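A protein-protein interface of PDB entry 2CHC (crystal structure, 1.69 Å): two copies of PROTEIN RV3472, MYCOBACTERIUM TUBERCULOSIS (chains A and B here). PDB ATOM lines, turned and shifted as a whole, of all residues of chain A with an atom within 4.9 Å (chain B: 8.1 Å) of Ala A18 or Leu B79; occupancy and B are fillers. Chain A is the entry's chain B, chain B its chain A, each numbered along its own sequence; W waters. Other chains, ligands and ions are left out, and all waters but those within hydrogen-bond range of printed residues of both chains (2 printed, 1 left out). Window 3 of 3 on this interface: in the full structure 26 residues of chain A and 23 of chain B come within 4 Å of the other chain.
The side-chain carboxylate of Asp B77 lies within hydrogen-bond range of the side-chain hydroxyl of Thr B76, at 3.0 Å.
The backbone carbonyl oxygen (O) of Arg B90 lies within hydrogen-bond range of the backbone NH (N) of Leu B79, at 2.9 Å.
Among the printed residues, merely in contact across the chains: Ala A21 with Asp B77 (3.5 Å), Leu A25 with Asp B77 (3.5 Å), Leu A25 with Arg B90 (3.5 Å), Ala A21 with Leu B78 (3.6 Å), Leu A14 with Trp B10 (3.6 Å), Leu A25 with Leu B79 (3.6 Å), Ala A18 with Leu B79 (3.8 Å), Arg A15 with Trp B10 (3.9 Å) and Ala A18 with Trp B10 (3.97 Å).
Ala A18 touches just these residues of chain B: Trp B10 (3.97 Å) and Leu B79 (3.8 Å).
Of the printed residues of chain A, Leu B79 touches Ala A18 (3.8 Å) and Leu A25 (3.6 Å).
Of the printed residues of chain B, Leu A25 touches Asp B77 (3.5 Å), Leu B79 (3.6 Å) and Arg B90 (3.5 Å).
Of the printed residues of chain A, Trp B10 touches Leu A14 (3.6 Å), Arg A15 (3.9 Å) and Ala A18 (3.97 Å).
The nearest residue of chain B that does not touch Ala A18 is Leu B78 (4.9 Å).
The nearest printed residue of chain A that does not touch Asp B77 is Cys A20 (5.4 Å).
Printed residues of chain B that touch a printed residue of chain A: Trp B10, Asp B77, Leu B78, Leu B79 and Arg B90.
Printed residues of chain A that touch a printed residue of chain B: Leu A14, Arg A15, Ala A18, Ala A21 and Leu A25.
Along chain A the printed residues that touch a printed residue of chain B span positions 14 to 25.
Positions printed for both chains: 16, 17 and 20.
Of the 9 pairs that touch across the chains among the printed residues, none has its exchanged pair printed and touching as well.
Water W1 bridges the side-chain amide nitrogen (NE2) of Gln A17 and the side-chain amide oxygen (OE1) of Gln B17.
Water W2 lies within hydrogen-bond range of the guanidinium group of Arg A15 (3.2 Å) and the indole nitrogen of Trp B10 (3.4 Å).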
ATOM      1  N   LEU A  14      10.562 -15.950  -9.081  1.00  0.00           N
ATOM      2  CA  LEU A  14       9.626 -16.511 -10.078  1.00  0.00           C
ATOM      3  C   LEU A  14      10.375 -16.816 -11.411  1.00  0.00           C
ATOM      4  O   LEU A  14      10.076 -17.807 -12.118  1.00  0.00           O
ATOM      5  CB  LEU A  14       8.446 -15.569 -10.271  1.00  0.00           C
ATOM      6  CG  LEU A  14       7.472 -15.511  -9.088  1.00  0.00           C
ATOM      7  CD1 LEU A  14       6.414 -14.492  -9.277  1.00  0.00           C
ATOM      8  CD2 LEU A  14       6.778 -16.823  -8.947  1.00  0.00           C
ATOM      9  N   ARG A  15      11.293 -15.944 -11.774  1.00  0.00           N
ATOM     10  CA  ARG A  15      12.079 -16.149 -12.975  1.00  0.00           C
ATOM     11  C   ARG A  15      12.916 -17.400 -12.854  1.00  0.00           C
ATOM     12  O   ARG A  15      13.077 -18.174 -13.804  1.00  0.00           O
ATOM     13  CB  ARG A  15      12.998 -14.948 -13.232  1.00  0.00           C
ATOM     14  CG  ARG A  15      12.281 -13.689 -13.604  1.00  0.00           C
ATOM     15  CD  ARG A  15      13.323 -12.590 -13.782  1.00  0.00           C
ATOM     16  NE  ARG A  15      12.652 -11.367 -14.222  1.00  0.00           N
ATOM     17  CZ  ARG A  15      12.778 -10.165 -13.684  1.00  0.00           C
ATOM     18  NH1 ARG A  15      12.105  -9.159 -14.236  1.00  0.00           N
ATOM     19  NH2 ARG A  15      13.531  -9.937 -12.613  1.00  0.00           N
ATOM     20  N   ILE A  16      13.494 -17.632 -11.664  1.00  0.00           N
ATOM     21  CA  ILE A  16      14.284 -18.854 -11.436  1.00  0.00           C
ATOM     22  C   ILE A  16      13.441 -20.104 -11.498  1.00  0.00           C
ATOM     23  O   ILE A  16      13.828 -21.140 -12.109  1.00  0.00           O
ATOM     24  CB  ILE A  16      15.062 -18.733 -10.119  1.00  0.00           C
ATOM     25  CG1 ILE A  16      16.200 -17.730 -10.297  1.00  0.00           C
ATOM     26  CG2 ILE A  16      15.538 -20.046  -9.667  1.00  0.00           C
ATOM     27  CD1 ILE A  16      16.773 -17.190  -8.970  1.00  0.00           C
ATOM     28  N   GLN A  17      12.230 -20.008 -10.951  1.00  0.00           N
ATOM     29  CA  GLN A  17      11.256 -21.076 -11.052  1.00  0.00           C
ATOM     30  C   GLN A  17      11.008 -21.440 -12.507  1.00  0.00           C
ATOM     31  O   GLN A  17      10.918 -22.615 -12.864  1.00  0.00           O
ATOM     32  CB  GLN A  17       9.986 -20.717 -10.331  1.00  0.00           C
ATOM     33  CG  GLN A  17      10.320 -20.700  -8.845  1.00  0.00           C
ATOM     34  CD  GLN A  17       9.204 -20.476  -7.903  1.00  0.00           C
ATOM     35  OE1 GLN A  17       9.435 -20.561  -6.656  1.00  0.00           O
ATOM     36  NE2 GLN A  17       8.013 -20.141  -8.426  1.00  0.00           N
ATOM     37  N   ALA A  18      10.871 -20.432 -13.331  1.00  0.00           N
ATOM     38  CA  ALA A  18      10.567 -20.664 -14.768  1.00  0.00           C
ATOM     39  C   ALA A  18      11.773 -21.286 -15.438  1.00  0.00           C
ATOM     40  O   ALA A  18      11.623 -22.111 -16.314  1.00  0.00           O
ATOM     41  CB  ALA A  18      10.204 -19.398 -15.443  1.00  0.00           C
ATOM     42  N   LEU A  19      12.981 -20.852 -15.069  1.00  0.00           N
ATOM     43  CA  LEU A  19      14.182 -21.548 -15.603  1.00  0.00           C
ATOM     44  C   LEU A  19      14.214 -23.009 -15.242  1.00  0.00           C
ATOM     45  O   LEU A  19      14.491 -23.892 -16.062  1.00  0.00           O
ATOM     46  CB  LEU A  19      15.433 -20.850 -15.082  1.00  0.00           C
ATOM     47  CG  LEU A  19      16.709 -21.599 -15.331  1.00  0.00           C
ATOM     48  CD1 LEU A  19      16.993 -21.709 -16.790  1.00  0.00           C
ATOM     49  CD2 LEU A  19      17.821 -20.808 -14.613  1.00  0.00           C
ATOM     50  N   CYS A  20      13.915 -23.309 -13.981  1.00  0.00           N
ATOM     51  CA  CYS A  20      13.859 -24.727 -13.567  1.00  0.00           C
ATOM     52  C   CYS A  20      12.816 -25.503 -14.355  1.00  0.00           C
ATOM     53  O   CYS A  20      13.063 -26.637 -14.727  1.00  0.00           O
ATOM     54  CB  CYS A  20      13.569 -24.761 -12.079  1.00  0.00           C
ATOM     55  SG  CYS A  20      14.975 -24.334 -11.005  1.00  0.00           S
ATOM     56  N   ALA A  21      11.689 -24.923 -14.585  1.00  0.00           N
ATOM     57  CA  ALA A  21      10.580 -25.551 -15.345  1.00  0.00           C
ATOM     58  C   ALA A  21      11.047 -25.823 -16.767  1.00  0.00           C
ATOM     59  O   ALA A  21      10.888 -26.918 -17.324  1.00  0.00           O
ATOM     60  CB  ALA A  21       9.332 -24.674 -15.351  1.00  0.00           C
ATOM     61  N   ARG A  22      11.697 -24.812 -17.352  1.00  0.00           N
ATOM     62  CA  ARG A  22      12.210 -24.951 -18.723  1.00  0.00           C
ATOM     63  C   ARG A  22      13.200 -26.046 -18.883  1.00  0.00           C
ATOM     64  O   ARG A  22      13.198 -26.770 -19.887  1.00  0.00           O
ATOM     65  CB  ARG A  22      12.722 -23.601 -19.277  1.00  0.00           C
ATOM     66  CG  ARG A  22      13.082 -23.600 -20.781  1.00  0.00           C
ATOM     67  CD  ARG A  22      13.731 -22.247 -21.144  1.00  0.00           C
ATOM     68  NE  ARG A  22      12.941 -21.263 -20.405  1.00  0.00           N
ATOM     69  CZ  ARG A  22      13.390 -20.352 -19.542  1.00  0.00           C
ATOM     70  NH1 ARG A  22      14.681 -20.138 -19.363  1.00  0.00           N
ATOM     71  NH2 ARG A  22      12.498 -19.598 -18.894  1.00  0.00           N
ATOM     72  N   LEU A  25      11.076 -29.246 -18.900  1.00  0.00           N
ATOM     73  CA  LEU A  25      10.179 -29.386 -20.055  1.00  0.00           C
ATOM     74  C   LEU A  25      10.924 -29.591 -21.371  1.00  0.00           C
ATOM     75  O   LEU A  25      10.447 -30.361 -22.218  1.00  0.00           O
ATOM     76  CB  LEU A  25       9.248 -28.167 -20.190  1.00  0.00           C
ATOM     77  CG  LEU A  25       8.215 -28.137 -19.073  1.00  0.00           C
ATOM     78  CD1 LEU A  25       7.650 -26.723 -19.053  1.00  0.00           C
ATOM     79  CD2 LEU A  25       7.072 -29.184 -19.174  1.00  0.00           C
ATOM     80  N   TRP B  10       3.699 -11.834 -13.966  1.00  0.00           N
ATOM     81  CA  TRP B  10       4.046 -12.720 -12.785  1.00  0.00           C
ATOM     82  C   TRP B  10       2.927 -12.867 -11.745  1.00  0.00           C
ATOM     83  O   TRP B  10       2.696 -13.981 -11.282  1.00  0.00           O
ATOM     84  CB  TRP B  10       5.400 -12.352 -12.127  1.00  0.00           C
ATOM     85  CG  TRP B  10       6.600 -12.571 -13.067  1.00  0.00           C
ATOM     86  CD1 TRP B  10       7.400 -11.621 -13.633  1.00  0.00           C
ATOM     87  CD2 TRP B  10       7.068 -13.822 -13.564  1.00  0.00           C
ATOM     88  NE1 TRP B  10       8.328 -12.202 -14.448  1.00  0.00           N
ATOM     89  CE2 TRP B  10       8.137 -13.554 -14.431  1.00  0.00           C
ATOM     90  CE3 TRP B  10       6.674 -15.141 -13.381  1.00  0.00           C
ATOM     91  CZ2 TRP B  10       8.843 -14.571 -15.100  1.00  0.00           C
ATOM     92  CZ3 TRP B  10       7.409 -16.183 -14.044  1.00  0.00           C
ATOM     93  CH2 TRP B  10       8.439 -15.888 -14.897  1.00  0.00           C
ATOM     94  N   ILE B  13       0.713 -15.291 -13.181  1.00  0.00           N
ATOM     95  CA  ILE B  13       1.304 -16.607 -13.076  1.00  0.00           C
ATOM     96  C   ILE B  13       1.066 -17.329 -11.723  1.00  0.00           C
ATOM     97  O   ILE B  13       0.683 -18.507 -11.656  1.00  0.00           O
ATOM     98  CB  ILE B  13       2.769 -16.610 -13.419  1.00  0.00           C
ATOM     99  CG1 ILE B  13       2.963 -16.392 -14.919  1.00  0.00           C
ATOM    100  CG2 ILE B  13       3.402 -17.934 -13.019  1.00  0.00           C
ATOM    101  CD1 ILE B  13       2.545 -17.567 -15.731  1.00  0.00           C
ATOM    102  N   ILE B  16      -2.407 -18.548 -11.823  1.00  0.00           N
ATOM    103  CA  ILE B  16      -2.505 -19.771 -12.633  1.00  0.00           C
ATOM    104  C   ILE B  16      -1.984 -20.986 -11.863  1.00  0.00           C
ATOM    105  O   ILE B  16      -2.583 -22.084 -11.897  1.00  0.00           O
ATOM    106  CB  ILE B  16      -1.720 -19.575 -13.988  1.00  0.00           C
ATOM    107  CG1 ILE B  16      -2.547 -18.644 -14.861  1.00  0.00           C
ATOM    108  CG2 ILE B  16      -1.435 -20.944 -14.623  1.00  0.00           C
ATOM    109  CD1 ILE B  16      -1.767 -18.069 -16.106  1.00  0.00           C
ATOM    110  N   GLN B  17      -0.916 -20.798 -11.088  1.00  0.00           N
ATOM    111  CA  GLN B  17      -0.435 -21.828 -10.194  1.00  0.00           C
ATOM    112  C   GLN B  17      -1.520 -22.298  -9.224  1.00  0.00           C
ATOM    113  O   GLN B  17      -1.700 -23.476  -8.975  1.00  0.00           O
ATOM    114  CB  GLN B  17       0.793 -21.340  -9.438  1.00  0.00           C
ATOM    115  CG  GLN B  17       1.976 -21.217 -10.369  1.00  0.00           C
ATOM    116  CD  GLN B  17       3.190 -20.673  -9.687  1.00  0.00           C
ATOM    117  OE1 GLN B  17       3.213 -20.444  -8.465  1.00  0.00           O
ATOM    118  NE2 GLN B  17       4.230 -20.459 -10.484  1.00  0.00           N
ATOM    119  N   CYS B  20      -3.996 -24.454 -11.038  1.00  0.00           N
ATOM    120  CA  CYS B  20      -3.428 -25.823 -11.215  1.00  0.00           C
ATOM    121  C   CYS B  20      -3.488 -26.653  -9.920  1.00  0.00           C
ATOM    122  O   CYS B  20      -3.816 -27.815  -9.957  1.00  0.00           O
ATOM    123  CB  CYS B  20      -1.991 -25.695 -11.698  1.00  0.00           C
ATOM    124  SG  CYS B  20      -1.845 -25.220 -13.429  1.00  0.00           S
ATOM    125  N   THR B  76       3.724 -29.805 -11.585  1.00  0.00           N
ATOM    126  CA  THR B  76       4.967 -29.094 -11.290  1.00  0.00           C
ATOM    127  C   THR B  76       5.527 -28.554 -12.604  1.00  0.00           C
ATOM    128  O   THR B  76       4.943 -28.733 -13.680  1.00  0.00           O
ATOM    129  CB  THR B  76       6.054 -30.039 -10.679  1.00  0.00           C
ATOM    130  OG1 THR B  76       6.477 -30.970 -11.688  1.00  0.00           O
ATOM    131  CG2 THR B  76       5.536 -30.862  -9.575  1.00  0.00           C
ATOM    132  N   ASP B  77       6.628 -27.825 -12.479  1.00  0.00           N
ATOM    133  CA  ASP B  77       7.341 -27.353 -13.645  1.00  0.00           C
ATOM    134  C   ASP B  77       6.425 -26.473 -14.534  1.00  0.00           C
ATOM    135  O   ASP B  77       6.387 -26.622 -15.768  1.00  0.00           O
ATOM    136  CB  ASP B  77       7.843 -28.509 -14.555  1.00  0.00           C
ATOM    137  CG  ASP B  77       8.628 -29.648 -13.889  1.00  0.00           C
ATOM    138  OD1 ASP B  77       8.820 -30.706 -14.667  1.00  0.00           O
ATOM    139  OD2 ASP B  77       8.987 -29.634 -12.711  1.00  0.00           O
ATOM    140  N   LEU B  78       5.657 -25.583 -13.933  1.00  0.00           N
ATOM    141  CA  LEU B  78       4.746 -24.749 -14.714  1.00  0.00           C
ATOM    142  C   LEU B  78       5.410 -23.685 -15.493  1.00  0.00           C
ATOM    143  O   LEU B  78       6.241 -22.898 -14.962  1.00  0.00           O
ATOM    144  CB  LEU B  78       3.721 -24.025 -13.796  1.00  0.00           C
ATOM    145  CG  LEU B  78       2.571 -24.864 -13.205  1.00  0.00           C
ATOM    146  CD1 LEU B  78       2.982 -26.001 -12.318  1.00  0.00           C
ATOM    147  CD2 LEU B  78       1.628 -23.889 -12.458  1.00  0.00           C
ATOM    148  N   LEU B  79       5.073 -23.600 -16.765  1.00  0.00           N
ATOM    149  CA  LEU B  79       5.636 -22.627 -17.666  1.00  0.00           C
ATOM    150  C   LEU B  79       4.554 -22.094 -18.604  1.00  0.00           C
ATOM    151  O   LEU B  79       4.098 -22.762 -19.525  1.00  0.00           O
ATOM    152  CB  LEU B  79       6.854 -23.220 -18.450  1.00  0.00           C
ATOM    153  CG  LEU B  79       7.752 -22.247 -19.210  1.00  0.00           C
ATOM    154  CD1 LEU B  79       8.458 -21.298 -18.312  1.00  0.00           C
ATOM    155  CD2 LEU B  79       8.767 -22.966 -20.050  1.00  0.00           C
ATOM    156  N   TYR B  80       4.097 -20.861 -18.318  1.00  0.00           N
ATOM    157  CA  TYR B  80       2.969 -20.225 -19.017  1.00  0.00           C
ATOM    158  C   TYR B  80       3.305 -18.879 -19.680  1.00  0.00           C
ATOM    159  O   TYR B  80       4.172 -18.138 -19.163  1.00  0.00           O
ATOM    160  CB  TYR B  80       1.784 -20.080 -18.052  1.00  0.00           C
ATOM    161  CG  TYR B  80       1.183 -21.407 -17.726  1.00  0.00           C
ATOM    162  CD1 TYR B  80       1.800 -22.274 -16.868  1.00  0.00           C
ATOM    163  CD2 TYR B  80       0.034 -21.839 -18.404  1.00  0.00           C
ATOM    164  CE1 TYR B  80       1.299 -23.541 -16.601  1.00  0.00           C
ATOM    165  CE2 TYR B  80      -0.513 -23.077 -18.095  1.00  0.00           C
ATOM    166  CZ  TYR B  80       0.144 -23.955 -17.266  1.00  0.00           C
ATOM    167  OH  TYR B  80      -0.246 -25.267 -16.983  1.00  0.00           O
ATOM    168  N   GLU B  81       2.685 -18.617 -20.815  1.00  0.00           N
ATOM    169  CA  GLU B  81       2.788 -17.338 -21.521  1.00  0.00           C
ATOM    170  C   GLU B  81       1.414 -16.658 -21.350  1.00  0.00           C
ATOM    171  O   GLU B  81       0.398 -17.158 -21.850  1.00  0.00           O
ATOM    172  CB  GLU B  81       3.098 -17.596 -22.967  1.00  0.00           C
ATOM    173  CG  GLU B  81       4.512 -18.083 -23.216  1.00  0.00           C
ATOM    174  N   VAL B  82       1.394 -15.513 -20.660  1.00  0.00           N
ATOM    175  CA  VAL B  82       0.144 -14.794 -20.400  1.00  0.00           C
ATOM    176  C   VAL B  82       0.026 -13.656 -21.409  1.00  0.00           C
ATOM    177  O   VAL B  82       0.973 -12.892 -21.565  1.00  0.00           O
ATOM    178  CB  VAL B  82       0.137 -14.228 -18.981  1.00  0.00           C
ATOM    179  CG1 VAL B  82      -1.071 -13.362 -18.755  1.00  0.00           C
ATOM    180  CG2 VAL B  82       0.248 -15.344 -17.918  1.00  0.00           C
ATOM    181  N   ALA B  87      -4.004 -17.333 -21.496  1.00  0.00           N
ATOM    182  CA  ALA B  87      -2.689 -17.887 -21.302  1.00  0.00           C
ATOM    183  C   ALA B  87      -2.563 -19.248 -21.941  1.00  0.00           C
ATOM    184  O   ALA B  87      -3.547 -19.986 -22.053  1.00  0.00           O
ATOM    185  CB  ALA B  87      -2.359 -18.000 -19.826  1.00  0.00           C
ATOM    186  N   THR B  88      -1.347 -19.581 -22.346  1.00  0.00           N
ATOM    187  CA  THR B  88      -1.019 -20.923 -22.862  1.00  0.00           C
ATOM    188  C   THR B  88       0.205 -21.407 -22.129  1.00  0.00           C
ATOM    189  O   THR B  88       1.122 -20.658 -21.830  1.00  0.00           O
ATOM    190  CB  THR B  88      -0.796 -20.930 -24.371  1.00  0.00           C
ATOM    191  OG1 THR B  88       0.304 -20.044 -24.696  1.00  0.00           O
ATOM    192  CG2 THR B  88      -2.034 -20.507 -25.064  1.00  0.00           C
ATOM    193  N   GLY B  89       0.264 -22.679 -21.834  1.00  0.00           N
ATOM    194  CA  GLY B  89       1.445 -23.158 -21.152  1.00  0.00           C
ATOM    195  C   GLY B  89       1.425 -24.647 -20.995  1.00  0.00           C
ATOM    196  O   GLY B  89       0.631 -25.352 -21.606  1.00  0.00           O
ATOM    197  N   ARG B  90       2.435 -25.089 -20.289  1.00  0.00           N
ATOM    198  CA  ARG B  90       2.702 -26.486 -20.078  1.00  0.00           C
ATOM    199  C   ARG B  90       3.124 -26.720 -18.656  1.00  0.00           C
ATOM    200  O   ARG B  90       3.676 -25.848 -18.015  1.00  0.00           O
ATOM    201  CB  ARG B  90       3.829 -26.962 -20.974  1.00  0.00           C
ATOM    202  CG  ARG B  90       3.559 -26.848 -22.469  1.00  0.00           C
ATOM    203  CD  ARG B  90       4.834 -26.686 -23.188  1.00  0.00           C
ATOM    204  NE  ARG B  90       5.505 -27.957 -23.278  1.00  0.00           N
ATOM    205  CZ  ARG B  90       6.828 -28.102 -23.450  1.00  0.00           C
ATOM    206  NH1 ARG B  90       7.657 -27.080 -23.555  1.00  0.00           N
ATOM    207  NH2 ARG B  90       7.331 -29.302 -23.504  1.00  0.00           N
ATOM    208  N   SER B  91       2.878 -27.928 -18.171  1.00  0.00           N
ATOM    209  CA  SER B  91       3.335 -28.322 -16.876  1.00  0.00           C
ATOM    210  C   SER B  91       3.451 -29.839 -16.834  1.00  0.00           C
ATOM    211  O   SER B  91       2.920 -30.574 -17.679  1.00  0.00           O
ATOM    212  CB  SER B  91       2.388 -27.830 -15.794  1.00  0.00           C
ATOM    213  OG  SER B  91       1.092 -28.267 -16.073  1.00  0.00           O
ATOM    214  N   ALA B  92       4.280 -30.299 -15.909  1.00  0.00           N
ATOM    215  CA  ALA B  92       4.487 -31.708 -15.656  1.00  0.00           C
ATOM    216  C   ALA B  92       3.396 -32.310 -14.781  1.00  0.00           C
ATOM    217  O   ALA B  92       3.033 -31.717 -13.797  1.00  0.00           O
ATOM    218  CB  ALA B  92       5.866 -31.950 -15.016  1.00  0.00           C
ATOM    219  N   TYR B 111       0.872 -31.648 -19.202  1.00  0.00           N
ATOM    220  CA  TYR B 111      -0.341 -30.879 -19.553  1.00  0.00           C
ATOM    221  C   TYR B 111      -0.015 -29.772 -20.485  1.00  0.00           C
ATOM    222  O   TYR B 111       0.976 -29.082 -20.283  1.00  0.00           O
ATOM    223  CB  TYR B 111      -0.965 -30.244 -18.334  1.00  0.00           C
ATOM    224  CG  TYR B 111      -1.518 -31.159 -17.245  1.00  0.00           C
ATOM    225  CD1 TYR B 111      -1.101 -31.025 -15.946  1.00  0.00           C
ATOM    226  CD2 TYR B 111      -2.462 -32.140 -17.525  1.00  0.00           C
ATOM    227  CE1 TYR B 111      -1.589 -31.868 -14.980  1.00  0.00           C
ATOM    228  CE2 TYR B 111      -2.997 -32.948 -16.532  1.00  0.00           C
ATOM    229  CZ  TYR B 111      -2.571 -32.794 -15.270  1.00  0.00           C
ATOM    230  OH  TYR B 111      -3.019 -33.656 -14.251  1.00  0.00           O
ATOM    231  N   GLN B 112      -0.835 -29.632 -21.540  1.00  0.00           N
ATOM    232  CA  GLN B 112      -0.749 -28.494 -22.432  1.00  0.00           C
ATOM    233  C   GLN B 112      -2.096 -27.788 -22.323  1.00  0.00           C
ATOM    234  O   GLN B 112      -3.165 -28.331 -22.690  1.00  0.00           O
ATOM    235  CB  GLN B 112      -0.543 -29.011 -23.866  1.00  0.00           C
ATOM    236  CG  GLN B 112       0.653 -29.944 -23.902  1.00  0.00           C
ATOM    237  CD  GLN B 112       0.891 -30.580 -25.254  1.00  0.00           C
ATOM    238  OE1 GLN B 112      -0.055 -30.858 -26.026  1.00  0.00           O
ATOM    239  NE2 GLN B 112       2.170 -30.823 -25.553  1.00  0.00           N
ATOM    240  N   ASP B 113      -2.026 -26.560 -21.855  1.00  0.00           N
ATOM    241  CA  ASP B 113      -3.177 -25.798 -21.445  1.00  0.00           C
ATOM    242  C   ASP B 113      -3.403 -24.524 -22.247  1.00  0.00           C
ATOM    243  O   ASP B 113      -2.470 -23.807 -22.608  1.00  0.00           O
ATOM    244  CB  ASP B 113      -2.985 -25.362 -19.985  1.00  0.00           C
ATOM    245  CG  ASP B 113      -3.006 -26.495 -19.017  1.00  0.00           C
ATOM    246  OD1 ASP B 113      -3.630 -27.532 -19.278  1.00  0.00           O
ATOM    247  OD2 ASP B 113      -2.431 -26.220 -17.902  1.00  0.00           O
HETATM  248  O   HOH W   1       5.633 -20.143  -7.248  1.00  0.00           O
HETATM  249  O   HOH W   2      10.753 -11.424 -16.761  1.00  0.00           O
